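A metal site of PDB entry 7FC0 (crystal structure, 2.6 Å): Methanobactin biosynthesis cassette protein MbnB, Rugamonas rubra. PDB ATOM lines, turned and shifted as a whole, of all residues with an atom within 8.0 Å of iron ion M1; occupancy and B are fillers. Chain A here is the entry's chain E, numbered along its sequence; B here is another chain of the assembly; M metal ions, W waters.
The side-chain amide oxygen (OD1) of Asn 167 sits close to the backbone carbonyl oxygen (O) of Asn 135, 3.2 Å away.
The backbone carbonyl oxygen (O) of Asp 209 lies within hydrogen-bond range of the backbone NH (N) of Ala 27 of chain B (3.3 Å).
The backbone carbonyl oxygen of Gly 196 is in hydrogen-bond range of the backbone NH of His 211, 2.9 Å away.
ND1 of His 211 is in hydrogen-bond range of N of Gly 26 of chain B.
ND1 of His 211 is in hydrogen-bond range of OD2 of Asp 242 (2.7 Å).
N of Asp 164 is in hydrogen-bond range of OD1 of Asn 135 (2.7 Å).
OG of Ser 166 lies within hydrogen-bond range of N of Gly 195 (2.8 Å).
The side-chain sulfur (SG) of Cys 170 is in hydrogen-bond range of the backbone carbonyl oxygen (O) of Ser 166, at 3.4 Å.
Merely in contact with iron ion M1: Asp 164, Ser 166 and Glu 240.
Within 4 Å of iron ion M1: Asp 164, Ser 166, Asn 167, Asp 209, His 211 and Glu 240.
Iron ion M1 is bound by the side-chain amide nitrogen of Asn 167, water W1, the side-chain carboxylate of Asp 209 and a ring nitrogen (NE2) of His 211.
Slightly farther from iron ion M1 lies OD2 of Asp 209 (2.8 Å).
Water W1 bridges the side-chain carboxylate (OD2) of Asp 209 (2.6 Å) and the side-chain amide oxygen (OD1) of Asn 167 (2.9 Å).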
ATOM      1  N   HIS A  90      34.375 -29.737   2.231  1.00  0.00           N
ATOM      2  CA  HIS A  90      33.979 -28.639   3.081  1.00  0.00           C
ATOM      3  C   HIS A  90      34.922 -28.520   4.271  1.00  0.00           C
ATOM      4  O   HIS A  90      35.435 -29.508   4.784  1.00  0.00           O
ATOM      5  CB  HIS A  90      32.540 -28.823   3.607  1.00  0.00           C
ATOM      6  CG  HIS A  90      31.488 -28.647   2.565  1.00  0.00           C
ATOM      7  ND1 HIS A  90      31.015 -29.695   1.804  1.00  0.00           N
ATOM      8  CD2 HIS A  90      30.801 -27.553   2.160  1.00  0.00           C
ATOM      9  CE1 HIS A  90      30.087 -29.249   0.991  1.00  0.00           C
ATOM     10  NE2 HIS A  90      29.952 -27.954   1.162  1.00  0.00           N
ATOM     11  N   GLU A 134      35.853 -25.539   0.142  1.00  0.00           N
ATOM     12  CA  GLU A 134      34.853 -24.486  -0.007  1.00  0.00           C
ATOM     13  C   GLU A 134      34.917 -23.496   1.150  1.00  0.00           C
ATOM     14  O   GLU A 134      34.997 -23.885   2.321  1.00  0.00           O
ATOM     15  CB  GLU A 134      33.443 -25.094  -0.074  1.00  0.00           C
ATOM     16  CG  GLU A 134      32.354 -24.083  -0.451  1.00  0.00           C
ATOM     17  CD  GLU A 134      31.037 -24.725  -0.801  1.00  0.00           C
ATOM     18  OE1 GLU A 134      30.866 -25.927  -0.559  1.00  0.00           O
ATOM     19  OE2 GLU A 134      30.136 -24.011  -1.293  1.00  0.00           O
ATOM     20  N   ASN A 135      34.848 -22.212   0.825  1.00  0.00           N
ATOM     21  CA  ASN A 135      34.684 -21.205   1.858  1.00  0.00           C
ATOM     22  C   ASN A 135      33.270 -21.240   2.436  1.00  0.00           C
ATOM     23  O   ASN A 135      32.309 -21.605   1.755  1.00  0.00           O
ATOM     24  CB  ASN A 135      34.979 -19.822   1.297  1.00  0.00           C
ATOM     25  CG  ASN A 135      34.183 -19.530   0.059  1.00  0.00           C
ATOM     26  OD1 ASN A 135      34.257 -20.266  -0.919  1.00  0.00           O
ATOM     27  ND2 ASN A 135      33.398 -18.450   0.073  1.00  0.00           N
ATOM     28  N   TYR A 136      33.154 -20.855   3.687  1.00  0.00           N
ATOM     29  CA  TYR A 136      31.988 -20.891   4.576  1.00  0.00           C
ATOM     30  C   TYR A 136      31.216 -19.581   4.484  1.00  0.00           C
ATOM     31  O   TYR A 136      31.817 -18.505   4.356  1.00  0.00           O
ATOM     32  CB  TYR A 136      32.421 -21.133   6.017  1.00  0.00           C
ATOM     33  CG  TYR A 136      31.309 -21.377   7.004  1.00  0.00           C
ATOM     34  CD1 TYR A 136      30.609 -20.311   7.592  1.00  0.00           C
ATOM     35  CD2 TYR A 136      30.965 -22.687   7.387  1.00  0.00           C
ATOM     36  CE1 TYR A 136      29.604 -20.531   8.504  1.00  0.00           C
ATOM     37  CE2 TYR A 136      29.954 -22.927   8.330  1.00  0.00           C
ATOM     38  CZ  TYR A 136      29.275 -21.832   8.872  1.00  0.00           C
ATOM     39  OH  TYR A 136      28.261 -22.024   9.791  1.00  0.00           O
ATOM     40  N   PRO A 137      29.892 -19.654   4.534  1.00  0.00           N
ATOM     41  CA  PRO A 137      29.062 -18.434   4.581  1.00  0.00           C
ATOM     42  C   PRO A 137      28.944 -17.819   5.974  1.00  0.00           C
ATOM     43  O   PRO A 137      27.994 -18.079   6.708  1.00  0.00           O
ATOM     44  CB  PRO A 137      27.707 -18.935   4.082  1.00  0.00           C
ATOM     45  CG  PRO A 137      27.663 -20.366   4.490  1.00  0.00           C
ATOM     46  CD  PRO A 137      29.089 -20.882   4.516  1.00  0.00           C
ATOM     47  N   ASP A 164      33.098 -20.259  -3.377  1.00  0.00           N
ATOM     48  CA  ASP A 164      31.668 -20.000  -3.502  1.00  0.00           C
ATOM     49  C   ASP A 164      31.443 -18.500  -3.394  1.00  0.00           C
ATOM     50  O   ASP A 164      31.495 -17.938  -2.296  1.00  0.00           O
ATOM     51  CB  ASP A 164      30.869 -20.746  -2.428  1.00  0.00           C
ATOM     52  CG  ASP A 164      29.357 -20.744  -2.687  1.00  0.00           C
ATOM     53  OD1 ASP A 164      28.796 -19.658  -2.925  1.00  0.00           O
ATOM     54  OD2 ASP A 164      28.728 -21.830  -2.646  1.00  0.00           O
ATOM     55  N   VAL A 165      31.175 -17.857  -4.533  1.00  0.00           N
ATOM     56  CA  VAL A 165      30.923 -16.413  -4.559  1.00  0.00           C
ATOM     57  C   VAL A 165      29.728 -16.051  -3.658  1.00  0.00           C
ATOM     58  O   VAL A 165      29.803 -15.100  -2.868  1.00  0.00           O
ATOM     59  CB  VAL A 165      30.664 -15.946  -5.997  1.00  0.00           C
ATOM     60  CG1 VAL A 165      30.456 -14.439  -6.030  1.00  0.00           C
ATOM     61  CG2 VAL A 165      31.796 -16.358  -6.889  1.00  0.00           C
ATOM     62  N   SER A 166      28.606 -16.780  -3.777  1.00  0.00           N
ATOM     63  CA  SER A 166      27.416 -16.440  -2.990  1.00  0.00           C
ATOM     64  C   SER A 166      27.675 -16.609  -1.489  1.00  0.00           C
ATOM     65  O   SER A 166      27.240 -15.770  -0.677  1.00  0.00           O
ATOM     66  CB  SER A 166      26.176 -17.217  -3.471  1.00  0.00           C
ATOM     67  OG  SER A 166      26.139 -18.613  -3.198  1.00  0.00           O
ATOM     68  N   ASN A 167      28.408 -17.654  -1.091  1.00  0.00           N
ATOM     69  CA  ASN A 167      28.752 -17.775   0.310  1.00  0.00           C
ATOM     70  C   ASN A 167      29.557 -16.579   0.794  1.00  0.00           C
ATOM     71  O   ASN A 167      29.401 -16.171   1.951  1.00  0.00           O
ATOM     72  CB  ASN A 167      29.555 -19.034   0.572  1.00  0.00           C
ATOM     73  CG  ASN A 167      28.728 -20.259   0.552  1.00  0.00           C
ATOM     74  OD1 ASN A 167      29.214 -21.343   0.873  1.00  0.00           O
ATOM     75  ND2 ASN A 167      27.469 -20.131   0.166  1.00  0.00           N
ATOM     76  N   ALA A 168      30.421 -16.009  -0.058  1.00  0.00           N
ATOM     77  CA  ALA A 168      31.202 -14.831   0.318  1.00  0.00           C
ATOM     78  C   ALA A 168      30.334 -13.572   0.390  1.00  0.00           C
ATOM     79  O   ALA A 168      30.618 -12.664   1.176  1.00  0.00           O
ATOM     80  CB  ALA A 168      32.359 -14.608  -0.654  1.00  0.00           C
ATOM     81  N   CYS A 170      27.216 -13.671   1.385  1.00  0.00           N
ATOM     82  CA  CYS A 170      26.554 -13.818   2.677  1.00  0.00           C
ATOM     83  C   CYS A 170      27.431 -13.325   3.810  1.00  0.00           C
ATOM     84  O   CYS A 170      26.971 -12.633   4.721  1.00  0.00           O
ATOM     85  CB  CYS A 170      26.209 -15.286   2.928  1.00  0.00           C
ATOM     86  SG  CYS A 170      24.973 -16.025   1.857  1.00  0.00           S
ATOM     87  N   HIS A 193      31.343 -21.789  -7.025  1.00  0.00           N
ATOM     88  CA  HIS A 193      29.927 -21.995  -6.741  1.00  0.00           C
ATOM     89  C   HIS A 193      29.227 -20.657  -6.696  1.00  0.00           C
ATOM     90  O   HIS A 193      29.808 -19.642  -6.313  1.00  0.00           O
ATOM     91  CB  HIS A 193      29.678 -22.667  -5.397  1.00  0.00           C
ATOM     92  CG  HIS A 193      29.827 -24.151  -5.422  1.00  0.00           C
ATOM     93  ND1 HIS A 193      29.601 -24.921  -4.311  1.00  0.00           N
ATOM     94  CD2 HIS A 193      30.201 -24.996  -6.410  1.00  0.00           C
ATOM     95  CE1 HIS A 193      29.837 -26.182  -4.607  1.00  0.00           C
ATOM     96  NE2 HIS A 193      30.202 -26.255  -5.880  1.00  0.00           N
ATOM     97  N   VAL A 194      27.928 -20.692  -6.980  1.00  0.00           N
ATOM     98  CA  VAL A 194      27.062 -19.549  -6.711  1.00  0.00           C
ATOM     99  C   VAL A 194      25.639 -20.062  -6.517  1.00  0.00           C
ATOM    100  O   VAL A 194      25.193 -21.000  -7.191  1.00  0.00           O
ATOM    101  CB  VAL A 194      27.150 -18.506  -7.855  1.00  0.00           C
ATOM    102  CG1 VAL A 194      26.518 -19.030  -9.110  1.00  0.00           C
ATOM    103  CG2 VAL A 194      26.512 -17.212  -7.413  1.00  0.00           C
ATOM    104  N   GLY A 195      24.946 -19.469  -5.548  1.00  0.00           N
ATOM    105  CA  GLY A 195      23.577 -19.846  -5.250  1.00  0.00           C
ATOM    106  C   GLY A 195      22.788 -18.692  -4.680  1.00  0.00           C
ATOM    107  O   GLY A 195      23.305 -17.595  -4.438  1.00  0.00           O
ATOM    108  N   GLY A 196      21.508 -18.947  -4.455  1.00  0.00           N
ATOM    109  CA  GLY A 196      20.663 -17.937  -3.873  1.00  0.00           C
ATOM    110  C   GLY A 196      20.826 -17.919  -2.380  1.00  0.00           C
ATOM    111  O   GLY A 196      21.341 -18.866  -1.785  1.00  0.00           O
ATOM    112  N   TYR A 197      20.427 -16.808  -1.752  1.00  0.00           N
ATOM    113  CA  TYR A 197      20.444 -16.721  -0.299  1.00  0.00           C
ATOM    114  C   TYR A 197      19.134 -16.095   0.200  1.00  0.00           C
ATOM    115  O   TYR A 197      18.285 -15.651  -0.578  1.00  0.00           O
ATOM    116  CB  TYR A 197      21.669 -15.960   0.184  1.00  0.00           C
ATOM    117  CG  TYR A 197      21.767 -14.558  -0.331  1.00  0.00           C
ATOM    118  CD1 TYR A 197      20.842 -13.600   0.063  1.00  0.00           C
ATOM    119  CD2 TYR A 197      22.816 -14.176  -1.157  1.00  0.00           C
ATOM    120  CE1 TYR A 197      20.925 -12.302  -0.381  1.00  0.00           C
ATOM    121  CE2 TYR A 197      22.897 -12.864  -1.602  1.00  0.00           C
ATOM    122  CZ  TYR A 197      21.940 -11.933  -1.215  1.00  0.00           C
ATOM    123  OH  TYR A 197      21.989 -10.624  -1.634  1.00  0.00           O
ATOM    124  N   VAL A 208      21.515 -15.903   5.085  1.00  0.00           N
ATOM    125  CA  VAL A 208      21.640 -17.348   5.255  1.00  0.00           C
ATOM    126  C   VAL A 208      21.806 -18.006   3.891  1.00  0.00           C
ATOM    127  O   VAL A 208      21.165 -17.625   2.910  1.00  0.00           O
ATOM    128  CB  VAL A 208      20.420 -17.911   5.988  1.00  0.00           C
ATOM    129  CG1 VAL A 208      20.510 -19.408   6.091  1.00  0.00           C
ATOM    130  CG2 VAL A 208      20.333 -17.305   7.388  1.00  0.00           C
ATOM    131  N   ASP A 209      22.657 -19.036   3.836  1.00  0.00           N
ATOM    132  CA  ASP A 209      23.077 -19.678   2.599  1.00  0.00           C
ATOM    133  C   ASP A 209      22.082 -20.786   2.225  1.00  0.00           C
ATOM    134  O   ASP A 209      22.299 -21.972   2.442  1.00  0.00           O
ATOM    135  CB  ASP A 209      24.497 -20.195   2.831  1.00  0.00           C
ATOM    136  CG  ASP A 209      25.037 -20.972   1.687  1.00  0.00           C
ATOM    137  OD1 ASP A 209      24.876 -20.529   0.539  1.00  0.00           O
ATOM    138  OD2 ASP A 209      25.661 -22.025   1.962  1.00  0.00           O
ATOM    139  N   THR A 210      20.963 -20.404   1.599  1.00  0.00           N
ATOM    140  CA  THR A 210      19.864 -21.359   1.480  1.00  0.00           C
ATOM    141  C   THR A 210      19.770 -22.072   0.134  1.00  0.00           C
ATOM    142  O   THR A 210      19.242 -23.178   0.095  1.00  0.00           O
ATOM    143  CB  THR A 210      18.523 -20.681   1.762  1.00  0.00           C
ATOM    144  OG1 THR A 210      18.387 -19.519   0.930  1.00  0.00           O
ATOM    145  CG2 THR A 210      18.474 -20.246   3.194  1.00  0.00           C
ATOM    146  N   HIS A 211      20.292 -21.487  -0.944  1.00  0.00           N
ATOM    147  CA  HIS A 211      20.207 -22.084  -2.282  1.00  0.00           C
ATOM    148  C   HIS A 211      18.758 -22.403  -2.648  1.00  0.00           C
ATOM    149  O   HIS A 211      18.460 -23.463  -3.212  1.00  0.00           O
ATOM    150  CB  HIS A 211      21.066 -23.346  -2.394  1.00  0.00           C
ATOM    151  CG  HIS A 211      22.449 -23.211  -1.861  1.00  0.00           C
ATOM    152  ND1 HIS A 211      23.179 -24.296  -1.419  1.00  0.00           N
ATOM    153  CD2 HIS A 211      23.247 -22.132  -1.709  1.00  0.00           C
ATOM    154  CE1 HIS A 211      24.370 -23.896  -1.007  1.00  0.00           C
ATOM    155  NE2 HIS A 211      24.433 -22.582  -1.173  1.00  0.00           N
ATOM    156  N   GLU A 240      23.994 -23.611  -7.580  1.00  0.00           N
ATOM    157  CA  GLU A 240      23.461 -24.494  -6.548  1.00  0.00           C
ATOM    158  C   GLU A 240      22.005 -24.132  -6.256  1.00  0.00           C
ATOM    159  O   GLU A 240      21.722 -23.022  -5.781  1.00  0.00           O
ATOM    160  CB  GLU A 240      24.265 -24.365  -5.253  1.00  0.00           C
ATOM    161  CG  GLU A 240      25.586 -25.061  -5.234  1.00  0.00           C
ATOM    162  CD  GLU A 240      26.363 -24.753  -3.976  1.00  0.00           C
ATOM    163  OE1 GLU A 240      26.763 -23.582  -3.769  1.00  0.00           O
ATOM    164  OE2 GLU A 240      26.561 -25.694  -3.174  1.00  0.00           O
ATOM    165  N   ASP A 242      19.098 -26.118  -3.987  1.00  0.00           N
ATOM    166  CA  ASP A 242      18.862 -27.279  -3.131  1.00  0.00           C
ATOM    167  C   ASP A 242      17.414 -27.458  -2.703  1.00  0.00           C
ATOM    168  O   ASP A 242      17.040 -28.554  -2.277  1.00  0.00           O
ATOM    169  CB  ASP A 242      19.716 -27.188  -1.854  1.00  0.00           C
ATOM    170  CG  ASP A 242      21.174 -27.454  -2.108  1.00  0.00           C
ATOM    171  OD1 ASP A 242      21.481 -28.394  -2.869  1.00  0.00           O
ATOM    172  OD2 ASP A 242      22.029 -26.726  -1.554  1.00  0.00           O
ATOM    173  N   CYS B  25      23.488 -29.050   0.735  1.00  0.00           N
ATOM    174  CA  CYS B  25      24.415 -28.030   1.219  1.00  0.00           C
ATOM    175  C   CYS B  25      23.712 -26.852   1.876  1.00  0.00           C
ATOM    176  O   CYS B  25      24.152 -26.348   2.913  1.00  0.00           O
ATOM    177  CB  CYS B  25      25.255 -27.506   0.074  1.00  0.00           C
ATOM    178  SG  CYS B  25      26.878 -28.192  -0.065  1.00  0.00           S
ATOM    179  N   GLY B  26      22.642 -26.355   1.258  1.00  0.00           N
ATOM    180  CA  GLY B  26      21.930 -25.229   1.805  1.00  0.00           C
ATOM    181  C   GLY B  26      21.217 -25.612   3.086  1.00  0.00           C
ATOM    182  O   GLY B  26      20.634 -26.694   3.201  1.00  0.00           O
ATOM    183  N   ALA B  27      21.303 -24.717   4.069  1.00  0.00           N
ATOM    184  CA  ALA B  27      20.513 -24.787   5.274  1.00  0.00           C
ATOM    185  C   ALA B  27      19.174 -24.102   5.022  1.00  0.00           C
ATOM    186  O   ALA B  27      19.011 -23.338   4.075  1.00  0.00           O
ATOM    187  CB  ALA B  27      21.230 -24.121   6.442  1.00  0.00           C
HETATM  188 FE    FE M   1      26.328 -21.438  -0.740  1.00  0.00          FE
HETATM  189 FE    FE M   2      28.519 -23.891  -2.333  1.00  0.00          FE
HETATM  190 FE    FE M   3      29.069 -26.934  -0.443  1.00  0.00          FE
HETATM  191  O   HOH W   1      27.098 -23.171   0.194  1.00  0.00           O
